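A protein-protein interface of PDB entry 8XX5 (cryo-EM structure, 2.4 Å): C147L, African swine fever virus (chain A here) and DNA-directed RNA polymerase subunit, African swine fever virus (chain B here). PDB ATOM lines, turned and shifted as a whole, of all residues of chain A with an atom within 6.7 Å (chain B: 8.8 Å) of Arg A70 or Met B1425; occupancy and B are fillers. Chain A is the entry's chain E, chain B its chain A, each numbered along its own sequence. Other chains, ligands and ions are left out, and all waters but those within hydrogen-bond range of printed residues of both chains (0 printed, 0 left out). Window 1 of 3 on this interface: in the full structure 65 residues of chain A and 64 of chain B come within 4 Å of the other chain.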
ATOM      1  N   THR A  64      24.947 -10.419  -6.081  1.00  0.00           N
ATOM      2  CA  THR A  64      24.040 -10.074  -7.160  1.00  0.00           C
ATOM      3  C   THR A  64      24.801  -9.313  -8.241  1.00  0.00           C
ATOM      4  O   THR A  64      25.890  -8.783  -8.010  1.00  0.00           O
ATOM      5  CB  THR A  64      22.867  -9.236  -6.647  1.00  0.00           C
ATOM      6  OG1 THR A  64      23.342  -7.968  -6.182  1.00  0.00           O
ATOM      7  CG2 THR A  64      22.162  -9.951  -5.507  1.00  0.00           C
ATOM      8  N   THR A  65      24.222  -9.276  -9.442  1.00  0.00           N
ATOM      9  CA  THR A  65      24.842  -8.504 -10.512  1.00  0.00           C
ATOM     10  C   THR A  65      24.941  -7.033 -10.140  1.00  0.00           C
ATOM     11  O   THR A  65      25.903  -6.359 -10.522  1.00  0.00           O
ATOM     12  CB  THR A  65      24.066  -8.676 -11.816  1.00  0.00           C
ATOM     13  OG1 THR A  65      22.661  -8.705 -11.538  1.00  0.00           O
ATOM     14  CG2 THR A  65      24.465  -9.971 -12.499  1.00  0.00           C
ATOM     15  N   PHE A  66      23.970  -6.526  -9.378  1.00  0.00           N
ATOM     16  CA  PHE A  66      24.055  -5.162  -8.870  1.00  0.00           C
ATOM     17  C   PHE A  66      25.254  -4.995  -7.946  1.00  0.00           C
ATOM     18  O   PHE A  66      26.035  -4.049  -8.087  1.00  0.00           O
ATOM     19  CB  PHE A  66      22.768  -4.798  -8.133  1.00  0.00           C
ATOM     20  CG  PHE A  66      21.558  -4.748  -9.013  1.00  0.00           C
ATOM     21  CD1 PHE A  66      21.657  -4.331 -10.327  1.00  0.00           C
ATOM     22  CD2 PHE A  66      20.318  -5.113  -8.522  1.00  0.00           C
ATOM     23  CE1 PHE A  66      20.545  -4.282 -11.134  1.00  0.00           C
ATOM     24  CE2 PHE A  66      19.202  -5.065  -9.325  1.00  0.00           C
ATOM     25  CZ  PHE A  66      19.315  -4.649 -10.633  1.00  0.00           C
ATOM     26  N   GLU A  67      25.417  -5.916  -6.993  1.00  0.00           N
ATOM     27  CA  GLU A  67      26.511  -5.808  -6.033  1.00  0.00           C
ATOM     28  C   GLU A  67      27.865  -5.970  -6.710  1.00  0.00           C
ATOM     29  O   GLU A  67      28.797  -5.211  -6.429  1.00  0.00           O
ATOM     30  CB  GLU A  67      26.342  -6.844  -4.925  1.00  0.00           C
ATOM     31  CG  GLU A  67      25.524  -6.359  -3.748  1.00  0.00           C
ATOM     32  CD  GLU A  67      24.797  -7.483  -3.042  1.00  0.00           C
ATOM     33  OE1 GLU A  67      25.006  -8.656  -3.413  1.00  0.00           O
ATOM     34  OE2 GLU A  67      24.015  -7.194  -2.114  1.00  0.00           O
ATOM     35  N   ALA A  68      27.995  -6.958  -7.597  1.00  0.00           N
ATOM     36  CA  ALA A  68      29.260  -7.157  -8.297  1.00  0.00           C
ATOM     37  C   ALA A  68      29.585  -5.969  -9.192  1.00  0.00           C
ATOM     38  O   ALA A  68      30.739  -5.527  -9.257  1.00  0.00           O
ATOM     39  CB  ALA A  68      29.210  -8.450  -9.110  1.00  0.00           C
ATOM     40  N   THR A  69      28.579  -5.435  -9.886  1.00  0.00           N
ATOM     41  CA  THR A  69      28.797  -4.266 -10.729  1.00  0.00           C
ATOM     42  C   THR A  69      29.228  -3.064  -9.901  1.00  0.00           C
ATOM     43  O   THR A  69      30.140  -2.327 -10.291  1.00  0.00           O
ATOM     44  CB  THR A  69      27.528  -3.946 -11.517  1.00  0.00           C
ATOM     45  OG1 THR A  69      27.114  -5.107 -12.246  1.00  0.00           O
ATOM     46  CG2 THR A  69      27.779  -2.815 -12.490  1.00  0.00           C
ATOM     47  N   ARG A  70      28.584  -2.848  -8.753  1.00  0.00           N
ATOM     48  CA  ARG A  70      28.962  -1.738  -7.887  1.00  0.00           C
ATOM     49  C   ARG A  70      30.373  -1.918  -7.341  1.00  0.00           C
ATOM     50  O   ARG A  70      31.138  -0.953  -7.255  1.00  0.00           O
ATOM     51  CB  ARG A  70      27.955  -1.596  -6.748  1.00  0.00           C
ATOM     52  CG  ARG A  70      28.359  -0.595  -5.688  1.00  0.00           C
ATOM     53  CD  ARG A  70      28.165   0.832  -6.152  1.00  0.00           C
ATOM     54  NE  ARG A  70      28.375   1.775  -5.061  1.00  0.00           N
ATOM     55  CZ  ARG A  70      28.546   3.079  -5.217  1.00  0.00           C
ATOM     56  NH1 ARG A  70      28.531   3.640  -6.414  1.00  0.00           N
ATOM     57  NH2 ARG A  70      28.740   3.841  -4.145  1.00  0.00           N
ATOM     58  N   LEU A  71      30.734  -3.146  -6.963  1.00  0.00           N
ATOM     59  CA  LEU A  71      32.084  -3.409  -6.479  1.00  0.00           C
ATOM     60  C   LEU A  71      33.119  -3.103  -7.553  1.00  0.00           C
ATOM     61  O   LEU A  71      34.135  -2.453  -7.287  1.00  0.00           O
ATOM     62  CB  LEU A  71      32.207  -4.862  -6.028  1.00  0.00           C
ATOM     63  CG  LEU A  71      31.596  -5.243  -4.684  1.00  0.00           C
ATOM     64  CD1 LEU A  71      31.376  -6.740  -4.633  1.00  0.00           C
ATOM     65  CD2 LEU A  71      32.486  -4.790  -3.545  1.00  0.00           C
ATOM     66  N   VAL A  72      32.867  -3.561  -8.781  1.00  0.00           N
ATOM     67  CA  VAL A  72      33.811  -3.317  -9.867  1.00  0.00           C
ATOM     68  C   VAL A  72      33.905  -1.828 -10.165  1.00  0.00           C
ATOM     69  O   VAL A  72      34.999  -1.295 -10.381  1.00  0.00           O
ATOM     70  CB  VAL A  72      33.415  -4.126 -11.117  1.00  0.00           C
ATOM     71  CG1 VAL A  72      34.277  -3.731 -12.302  1.00  0.00           C
ATOM     72  CG2 VAL A  72      33.550  -5.611 -10.843  1.00  0.00           C
ATOM     73  N   ALA A  73      32.768  -1.129 -10.175  1.00  0.00           N
ATOM     74  CA  ALA A  73      32.782   0.301 -10.466  1.00  0.00           C
ATOM     75  C   ALA A  73      33.533   1.078  -9.394  1.00  0.00           C
ATOM     76  O   ALA A  73      34.330   1.970  -9.708  1.00  0.00           O
ATOM     77  CB  ALA A  73      31.354   0.822 -10.606  1.00  0.00           C
ATOM     78  N   VAL A  74      33.302   0.747  -8.122  1.00  0.00           N
ATOM     79  CA  VAL A  74      33.989   1.432  -7.032  1.00  0.00           C
ATOM     80  C   VAL A  74      35.485   1.162  -7.096  1.00  0.00           C
ATOM     81  O   VAL A  74      36.306   2.077  -6.961  1.00  0.00           O
ATOM     82  CB  VAL A  74      33.392   1.009  -5.677  1.00  0.00           C
ATOM     83  CG1 VAL A  74      34.318   1.399  -4.537  1.00  0.00           C
ATOM     84  CG2 VAL A  74      32.020   1.627  -5.488  1.00  0.00           C
ATOM     85  N   ARG A  75      35.863  -0.100  -7.314  1.00  0.00           N
ATOM     86  CA  ARG A  75      37.276  -0.448  -7.384  1.00  0.00           C
ATOM     87  C   ARG A  75      37.961   0.241  -8.557  1.00  0.00           C
ATOM     88  O   ARG A  75      39.085   0.733  -8.423  1.00  0.00           O
ATOM     89  CB  ARG A  75      37.434  -1.965  -7.481  1.00  0.00           C
ATOM     90  CG  ARG A  75      38.865  -2.448  -7.372  1.00  0.00           C
ATOM     91  CD  ARG A  75      39.515  -1.969  -6.089  1.00  0.00           C
ATOM     92  NE  ARG A  75      40.961  -2.151  -6.122  1.00  0.00           N
ATOM     93  CZ  ARG A  75      41.837  -1.291  -5.622  1.00  0.00           C
ATOM     94  NH1 ARG A  75      41.447  -0.176  -5.028  1.00  0.00           N
ATOM     95  NH2 ARG A  75      43.136  -1.558  -5.720  1.00  0.00           N
ATOM     96  N   LEU A 109      37.353  -4.436  -1.043  1.00  0.00           N
ATOM     97  CA  LEU A 109      36.086  -3.888  -0.589  1.00  0.00           C
ATOM     98  C   LEU A 109      35.259  -4.950   0.124  1.00  0.00           C
ATOM     99  O   LEU A 109      35.505  -6.151   0.004  1.00  0.00           O
ATOM    100  CB  LEU A 109      35.297  -3.313  -1.765  1.00  0.00           C
ATOM    101  CG  LEU A 109      36.049  -2.342  -2.673  1.00  0.00           C
ATOM    102  CD1 LEU A 109      35.432  -2.314  -4.058  1.00  0.00           C
ATOM    103  CD2 LEU A 109      36.064  -0.954  -2.064  1.00  0.00           C
ATOM    104  N   TYR B   5      30.206  14.323   4.347  1.00  0.00           N
ATOM    105  CA  TYR B   5      29.220  13.736   3.451  1.00  0.00           C
ATOM    106  C   TYR B   5      27.964  13.345   4.218  1.00  0.00           C
ATOM    107  O   TYR B   5      28.032  12.830   5.337  1.00  0.00           O
ATOM    108  CB  TYR B   5      29.812  12.515   2.750  1.00  0.00           C
ATOM    109  CG  TYR B   5      28.838  11.757   1.882  1.00  0.00           C
ATOM    110  CD1 TYR B   5      28.583  12.157   0.581  1.00  0.00           C
ATOM    111  CD2 TYR B   5      28.179  10.636   2.362  1.00  0.00           C
ATOM    112  CE1 TYR B   5      27.699  11.463  -0.216  1.00  0.00           C
ATOM    113  CE2 TYR B   5      27.295   9.939   1.575  1.00  0.00           C
ATOM    114  CZ  TYR B   5      27.058  10.355   0.286  1.00  0.00           C
ATOM    115  OH  TYR B   5      26.175   9.659  -0.503  1.00  0.00           O
ATOM    116  N   GLU B   7      23.435  12.309   3.592  1.00  0.00           N
ATOM    117  CA  GLU B   7      22.314  11.976   2.728  1.00  0.00           C
ATOM    118  C   GLU B   7      21.021  12.354   3.433  1.00  0.00           C
ATOM    119  O   GLU B   7      20.903  12.202   4.651  1.00  0.00           O
ATOM    120  CB  GLU B   7      22.299  10.484   2.374  1.00  0.00           C
ATOM    121  CG  GLU B   7      23.330  10.076   1.337  1.00  0.00           C
ATOM    122  CD  GLU B   7      23.306   8.588   1.050  1.00  0.00           C
ATOM    123  OE1 GLU B   7      22.201   8.009   1.000  1.00  0.00           O
ATOM    124  OE2 GLU B   7      24.391   7.994   0.876  1.00  0.00           O
ATOM    125  N   MET B 472      32.703   4.629 -13.491  1.00  0.00           N
ATOM    126  CA  MET B 472      31.605   3.855 -12.918  1.00  0.00           C
ATOM    127  C   MET B 472      30.506   3.608 -13.943  1.00  0.00           C
ATOM    128  O   MET B 472      29.980   2.492 -14.051  1.00  0.00           O
ATOM    129  CB  MET B 472      31.036   4.574 -11.696  1.00  0.00           C
ATOM    130  CG  MET B 472      32.009   4.745 -10.546  1.00  0.00           C
ATOM    131  SD  MET B 472      31.152   4.723  -8.962  1.00  0.00           S
ATOM    132  CE  MET B 472      32.501   5.021  -7.831  1.00  0.00           C
ATOM    133  N   SER B 473      30.155   4.641 -14.711  1.00  0.00           N
ATOM    134  CA  SER B 473      29.119   4.492 -15.725  1.00  0.00           C
ATOM    135  C   SER B 473      29.548   3.516 -16.812  1.00  0.00           C
ATOM    136  O   SER B 473      28.731   2.735 -17.303  1.00  0.00           O
ATOM    137  CB  SER B 473      28.774   5.852 -16.326  1.00  0.00           C
ATOM    138  OG  SER B 473      27.545   5.800 -17.026  1.00  0.00           O
ATOM    139  N   VAL B 475      31.728   0.978 -16.448  1.00  0.00           N
ATOM    140  CA  VAL B 475      31.669  -0.342 -15.828  1.00  0.00           C
ATOM    141  C   VAL B 475      30.242  -0.863 -15.861  1.00  0.00           C
ATOM    142  O   VAL B 475      29.981  -2.010 -16.244  1.00  0.00           O
ATOM    143  CB  VAL B 475      32.197  -0.282 -14.383  1.00  0.00           C
ATOM    144  CG1 VAL B 475      31.731  -1.496 -13.596  1.00  0.00           C
ATOM    145  CG2 VAL B 475      33.701  -0.175 -14.362  1.00  0.00           C
ATOM    146  N   GLU B 476      29.298  -0.013 -15.472  1.00  0.00           N
ATOM    147  CA  GLU B 476      27.905  -0.424 -15.418  1.00  0.00           C
ATOM    148  C   GLU B 476      27.341  -0.696 -16.806  1.00  0.00           C
ATOM    149  O   GLU B 476      26.555  -1.632 -16.991  1.00  0.00           O
ATOM    150  CB  GLU B 476      27.101   0.655 -14.729  1.00  0.00           C
ATOM    151  CG  GLU B 476      26.195   0.141 -13.688  1.00  0.00           C
ATOM    152  CD  GLU B 476      25.360   1.240 -13.171  1.00  0.00           C
ATOM    153  OE1 GLU B 476      24.535   1.725 -13.961  1.00  0.00           O
ATOM    154  OE2 GLU B 476      25.559   1.645 -12.009  1.00  0.00           O
ATOM    155  N   LEU B 479      28.630  -3.980 -17.894  1.00  0.00           N
ATOM    156  CA  LEU B 479      28.337  -5.069 -16.974  1.00  0.00           C
ATOM    157  C   LEU B 479      26.857  -5.267 -16.688  1.00  0.00           C
ATOM    158  O   LEU B 479      26.467  -6.370 -16.291  1.00  0.00           O
ATOM    159  CB  LEU B 479      29.056  -4.844 -15.636  1.00  0.00           C
ATOM    160  CG  LEU B 479      30.461  -5.420 -15.481  1.00  0.00           C
ATOM    161  CD1 LEU B 479      30.902  -5.321 -14.031  1.00  0.00           C
ATOM    162  CD2 LEU B 479      30.509  -6.858 -15.963  1.00  0.00           C
ATOM    163  N   LEU B 480      26.037  -4.253 -16.868  1.00  0.00           N
ATOM    164  CA  LEU B 480      24.649  -4.335 -16.430  1.00  0.00           C
ATOM    165  C   LEU B 480      23.645  -4.017 -17.525  1.00  0.00           C
ATOM    166  O   LEU B 480      22.585  -4.644 -17.574  1.00  0.00           O
ATOM    167  CB  LEU B 480      24.437  -3.382 -15.244  1.00  0.00           C
ATOM    168  CG  LEU B 480      23.329  -3.709 -14.248  1.00  0.00           C
ATOM    169  CD1 LEU B 480      23.722  -4.885 -13.372  1.00  0.00           C
ATOM    170  CD2 LEU B 480      23.023  -2.487 -13.404  1.00  0.00           C
ATOM    171  N   TYR B 840      16.366  -7.770   0.841  1.00  0.00           N
ATOM    172  CA  TYR B 840      17.363  -8.813   1.054  1.00  0.00           C
ATOM    173  C   TYR B 840      16.747 -10.162   1.391  1.00  0.00           C
ATOM    174  O   TYR B 840      17.440 -11.180   1.313  1.00  0.00           O
ATOM    175  CB  TYR B 840      18.330  -8.386   2.153  1.00  0.00           C
ATOM    176  CG  TYR B 840      19.243  -7.266   1.727  1.00  0.00           C
ATOM    177  CD1 TYR B 840      20.082  -7.411   0.633  1.00  0.00           C
ATOM    178  CD2 TYR B 840      19.256  -6.061   2.410  1.00  0.00           C
ATOM    179  CE1 TYR B 840      20.913  -6.390   0.237  1.00  0.00           C
ATOM    180  CE2 TYR B 840      20.083  -5.035   2.021  1.00  0.00           C
ATOM    181  CZ  TYR B 840      20.910  -5.203   0.936  1.00  0.00           C
ATOM    182  OH  TYR B 840      21.736  -4.180   0.548  1.00  0.00           O
ATOM    183  N   TYR B1037      18.664  -8.535  -5.307  1.00  0.00           N
ATOM    184  CA  TYR B1037      18.298  -7.582  -4.270  1.00  0.00           C
ATOM    185  C   TYR B1037      18.321  -6.168  -4.832  1.00  0.00           C
ATOM    186  O   TYR B1037      19.234  -5.792  -5.571  1.00  0.00           O
ATOM    187  CB  TYR B1037      19.256  -7.682  -3.084  1.00  0.00           C
ATOM    188  CG  TYR B1037      19.420  -9.068  -2.511  1.00  0.00           C
ATOM    189  CD1 TYR B1037      18.319  -9.863  -2.240  1.00  0.00           C
ATOM    190  CD2 TYR B1037      20.679  -9.573  -2.222  1.00  0.00           C
ATOM    191  CE1 TYR B1037      18.467 -11.124  -1.707  1.00  0.00           C
ATOM    192  CE2 TYR B1037      20.836 -10.833  -1.689  1.00  0.00           C
ATOM    193  CZ  TYR B1037      19.727 -11.604  -1.434  1.00  0.00           C
ATOM    194  OH  TYR B1037      19.877 -12.863  -0.902  1.00  0.00           O
ATOM    195  N   GLY B1038      17.313  -5.380  -4.477  1.00  0.00           N
ATOM    196  CA  GLY B1038      17.239  -4.015  -4.946  1.00  0.00           C
ATOM    197  C   GLY B1038      16.693  -3.836  -6.341  1.00  0.00           C
ATOM    198  O   GLY B1038      16.872  -2.762  -6.923  1.00  0.00           O
ATOM    199  N   SER B1418      18.669  13.616  -5.081  1.00  0.00           N
ATOM    200  CA  SER B1418      19.479  12.459  -4.753  1.00  0.00           C
ATOM    201  C   SER B1418      19.207  11.337  -5.749  1.00  0.00           C
ATOM    202  O   SER B1418      18.511  11.514  -6.752  1.00  0.00           O
ATOM    203  CB  SER B1418      19.202  12.021  -3.315  1.00  0.00           C
ATOM    204  OG  SER B1418      20.043  10.943  -2.944  1.00  0.00           O
ATOM    205  N   VAL B1419      19.763  10.163  -5.472  1.00  0.00           N
ATOM    206  CA  VAL B1419      19.592   8.998  -6.331  1.00  0.00           C
ATOM    207  C   VAL B1419      18.828   7.936  -5.551  1.00  0.00           C
ATOM    208  O   VAL B1419      19.030   7.801  -4.337  1.00  0.00           O
ATOM    209  CB  VAL B1419      20.946   8.459  -6.816  1.00  0.00           C
ATOM    210  CG1 VAL B1419      20.895   8.150  -8.304  1.00  0.00           C
ATOM    211  CG2 VAL B1419      22.053   9.449  -6.501  1.00  0.00           C
ATOM    212  N   PRO B1420      17.938   7.181  -6.190  1.00  0.00           N
ATOM    213  CA  PRO B1420      17.263   6.088  -5.481  1.00  0.00           C
ATOM    214  C   PRO B1420      18.263   5.049  -4.994  1.00  0.00           C
ATOM    215  O   PRO B1420      19.246   4.741  -5.670  1.00  0.00           O
ATOM    216  CB  PRO B1420      16.318   5.509  -6.540  1.00  0.00           C
ATOM    217  CG  PRO B1420      16.129   6.611  -7.522  1.00  0.00           C
ATOM    218  CD  PRO B1420      17.423   7.355  -7.556  1.00  0.00           C
ATOM    219  N   ARG B1421      17.999   4.508  -3.807  1.00  0.00           N
ATOM    220  CA  ARG B1421      18.864   3.491  -3.211  1.00  0.00           C
ATOM    221  C   ARG B1421      18.377   2.105  -3.634  1.00  0.00           C
ATOM    222  O   ARG B1421      17.891   1.300  -2.840  1.00  0.00           O
ATOM    223  CB  ARG B1421      18.898   3.643  -1.695  1.00  0.00           C
ATOM    224  CG  ARG B1421      19.875   2.714  -0.991  1.00  0.00           C
ATOM    225  CD  ARG B1421      19.927   2.975   0.502  1.00  0.00           C
ATOM    226  NE  ARG B1421      19.867   4.397   0.814  1.00  0.00           N
ATOM    227  CZ  ARG B1421      20.838   5.071   1.414  1.00  0.00           C
ATOM    228  NH1 ARG B1421      21.964   4.482   1.780  1.00  0.00           N
ATOM    229  NH2 ARG B1421      20.674   6.369   1.655  1.00  0.00           N
ATOM    230  N   ILE B1422      18.504   1.842  -4.934  1.00  0.00           N
ATOM    231  CA  ILE B1422      18.141   0.560  -5.521  1.00  0.00           C
ATOM    232  C   ILE B1422      19.173   0.208  -6.583  1.00  0.00           C
ATOM    233  O   ILE B1422      20.035   1.013  -6.937  1.00  0.00           O
ATOM    234  CB  ILE B1422      16.726   0.567  -6.138  1.00  0.00           C
ATOM    235  CG1 ILE B1422      16.590   1.691  -7.158  1.00  0.00           C
ATOM    236  CG2 ILE B1422      15.679   0.725  -5.064  1.00  0.00           C
ATOM    237  CD1 ILE B1422      16.561   1.184  -8.569  1.00  0.00           C
ATOM    238  N   GLY B1423      19.064  -1.011  -7.102  1.00  0.00           N
ATOM    239  CA  GLY B1423      19.995  -1.454  -8.125  1.00  0.00           C
ATOM    240  C   GLY B1423      21.404  -1.530  -7.579  1.00  0.00           C
ATOM    241  O   GLY B1423      21.667  -2.181  -6.563  1.00  0.00           O
ATOM    242  N   THR B1424      22.331  -0.857  -8.262  1.00  0.00           N
ATOM    243  CA  THR B1424      23.716  -0.839  -7.809  1.00  0.00           C
ATOM    244  C   THR B1424      23.884  -0.135  -6.469  1.00  0.00           C
ATOM    245  O   THR B1424      24.834  -0.441  -5.741  1.00  0.00           O
ATOM    246  CB  THR B1424      24.607  -0.172  -8.858  1.00  0.00           C
ATOM    247  OG1 THR B1424      24.060   1.102  -9.215  1.00  0.00           O
ATOM    248  CG2 THR B1424      24.703  -1.039 -10.099  1.00  0.00           C
ATOM    249  N   MET B1425      22.989   0.786  -6.119  1.00  0.00           N
ATOM    250  CA  MET B1425      23.076   1.511  -4.859  1.00  0.00           C
ATOM    251  C   MET B1425      22.283   0.868  -3.734  1.00  0.00           C
ATOM    252  O   MET B1425      22.272   1.409  -2.626  1.00  0.00           O
ATOM    253  CB  MET B1425      22.605   2.955  -5.034  1.00  0.00           C
ATOM    254  CG  MET B1425      23.177   3.641  -6.236  1.00  0.00           C
ATOM    255  SD  MET B1425      24.902   4.073  -5.989  1.00  0.00           S
ATOM    256  CE  MET B1425      25.175   5.079  -7.432  1.00  0.00           C
ATOM    257  N   TYR B1426      21.618  -0.259  -3.984  1.00  0.00           N
ATOM    258  CA  TYR B1426      20.838  -0.883  -2.922  1.00  0.00           C
ATOM    259  C   TYR B1426      21.731  -1.358  -1.785  1.00  0.00           C
ATOM    260  O   TYR B1426      21.394  -1.186  -0.608  1.00  0.00           O
ATOM    261  CB  TYR B1426      20.014  -2.043  -3.477  1.00  0.00           C
ATOM    262  CG  TYR B1426      19.028  -2.567  -2.469  1.00  0.00           C
ATOM    263  CD1 TYR B1426      17.952  -1.793  -2.064  1.00  0.00           C
ATOM    264  CD2 TYR B1426      19.182  -3.822  -1.905  1.00  0.00           C
ATOM    265  CE1 TYR B1426      17.054  -2.256  -1.137  1.00  0.00           C
ATOM    266  CE2 TYR B1426      18.284  -4.297  -0.976  1.00  0.00           C
ATOM    267  CZ  TYR B1426      17.223  -3.507  -0.595  1.00  0.00           C
ATOM    268  OH  TYR B1426      16.323  -3.965   0.334  1.00  0.00           O
ATOM    269  N   SER B1427      22.872  -1.954  -2.113  1.00  0.00           N
ATOM    270  CA  SER B1427      23.845  -2.397  -1.126  1.00  0.00           C
ATOM    271  C   SER B1427      25.030  -1.445  -1.130  1.00  0.00           C
ATOM    272  O   SER B1427      25.554  -1.103  -2.195  1.00  0.00           O
ATOM    273  CB  SER B1427      24.313  -3.824  -1.413  1.00  0.00           C
ATOM    274  OG  SER B1427      23.277  -4.759  -1.176  1.00  0.00           O
ATOM    275  N   ASP B1428      25.446  -1.017   0.055  1.00  0.00           N
ATOM    276  CA  ASP B1428      26.571  -0.106   0.170  1.00  0.00           C
ATOM    277  C   ASP B1428      27.878  -0.882   0.281  1.00  0.00           C
ATOM    278  O   ASP B1428      27.907  -2.057   0.653  1.00  0.00           O
ATOM    279  CB  ASP B1428      26.410   0.811   1.378  1.00  0.00           C
ATOM    280  CG  ASP B1428      26.131   0.050   2.642  1.00  0.00           C
ATOM    281  OD1 ASP B1428      24.953  -0.278   2.894  1.00  0.00           O
ATOM    282  OD2 ASP B1428      27.095  -0.220   3.384  1.00  0.00           O
ATOM    283  N   ILE B1429      28.967  -0.197  -0.049  1.00  0.00           N
ATOM    284  CA  ILE B1429      30.301  -0.781  -0.085  1.00  0.00           C
ATOM    285  C   ILE B1429      31.155  -0.099   0.972  1.00  0.00           C
ATOM    286  O   ILE B1429      31.152   1.132   1.084  1.00  0.00           O
ATOM    287  CB  ILE B1429      30.937  -0.636  -1.477  1.00  0.00           C
ATOM    288  CG1 ILE B1429      29.973  -1.129  -2.556  1.00  0.00           C
ATOM    289  CG2 ILE B1429      32.249  -1.391  -1.543  1.00  0.00           C
ATOM    290  CD1 ILE B1429      29.655  -2.599  -2.468  1.00  0.00           C
ATOM    291  N   ILE B1430      31.876  -0.900   1.752  1.00  0.00           N
ATOM    292  CA  ILE B1430      32.838  -0.399   2.719  1.00  0.00           C
ATOM    293  C   ILE B1430      34.196  -1.005   2.391  1.00  0.00           C
ATOM    294  O   ILE B1430      34.300  -2.010   1.685  1.00  0.00           O
ATOM    295  CB  ILE B1430      32.431  -0.713   4.173  1.00  0.00           C
ATOM    296  CG1 ILE B1430      32.748  -2.168   4.517  1.00  0.00           C
ATOM    297  CG2 ILE B1430      30.958  -0.431   4.386  1.00  0.00           C
ATOM    298  CD1 ILE B1430      32.060  -2.666   5.766  1.00  0.00           C
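Of the 24 printed residues of chain B, 13 touch a printed residue of chain A.
Printed residues of chain B that touch a printed residue of chain A: Met B472, Val B475, Glu B476, Leu B479, Leu B480, Tyr B840, Tyr B1037, Gly B1423, Thr B1424, Met B1425, Ser B1427, Ile B1429 and Ile B1430.
Hydrophobic or aromatic side chains of chain B that line the printed part of chain A: Met B472, Val B475, Leu B479, Leu B480, Tyr B840, Tyr B1037, Met B1425 and Ile B1429.
Of the 13 printed residues of chain A, 11 touch a printed residue of chain B.
Hydrophobic or aromatic side chains of chain A that line the printed part of chain B: Phe A66, Leu A71, Val A72, Ala A73 and Leu A109.
OH of Tyr B840 is in hydrogen-bond range of O of Tyr B1426 (3.2 Å).
OG1 of Thr A64 sits at hydrogen-bond distance from N of Glu A67 (3.0 Å).
The backbone carbonyl oxygen (O) of Gly B1038 is in hydrogen-bond range of the backbone NH (N) of Gly B1423.
The side-chain hydroxyl of Thr A69 lies within hydrogen-bond range of the backbone carbonyl oxygen of Thr A65 (2.5 Å).
The side-chain carboxylate (OE2) of Glu B476 lies within hydrogen-bond range of the side-chain hydroxyl (OG1) of Thr B1424.
Of the printed residues of chain B, Arg A70 touches Met B472 (3.8 Å), Thr B1424 (3.5 Å), Met B1425 (3.7 Å) and Ile B1429 (3.6 Å).
Of the printed residues of chain A, Met B1425 touches Arg A70.
Thr A69 touches four residues of chain B.
Printed residues of chain A within 4 Å of Glu B476: Thr A69 (3.6 Å).
Of the printed residues of chain A, Leu B479 touches Thr A69.
Of the printed residues of chain B, Val A72 touches Val B475 (3.6 Å).
Ala A68 touches none of the printed residues of chain B.
NH1 of Arg A70 lies within hydrogen-bond range of SD of Met B1425 (3.7 Å).
The side-chain carboxylate of Glu A67 lies within hydrogen-bond range of the side-chain hydroxyl of Ser B1427 (2.7 Å).
Tyr B1037 touches Thr A64 (CD2 to CG2, 3.6 Å).
CD1 of Leu B480 touches O of Thr A65, at 3.9 Å.
Gly B1423 touches Phe A66.
Thr B1424 touches Phe A66.
Val B475 touches Thr A69.
CD1 of Ile B1429 touches CD2 of Leu A71, at 3.7 Å.
CG1 of Val A72 touches CG1 of Val B475 (3.6 Å).
Ala A73 touches Met B472.
CA of Val A74 touches CE of Met B472, at 3.97 Å.
CA of Leu A109 touches O of Ile B1430, 3.4 Å away.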
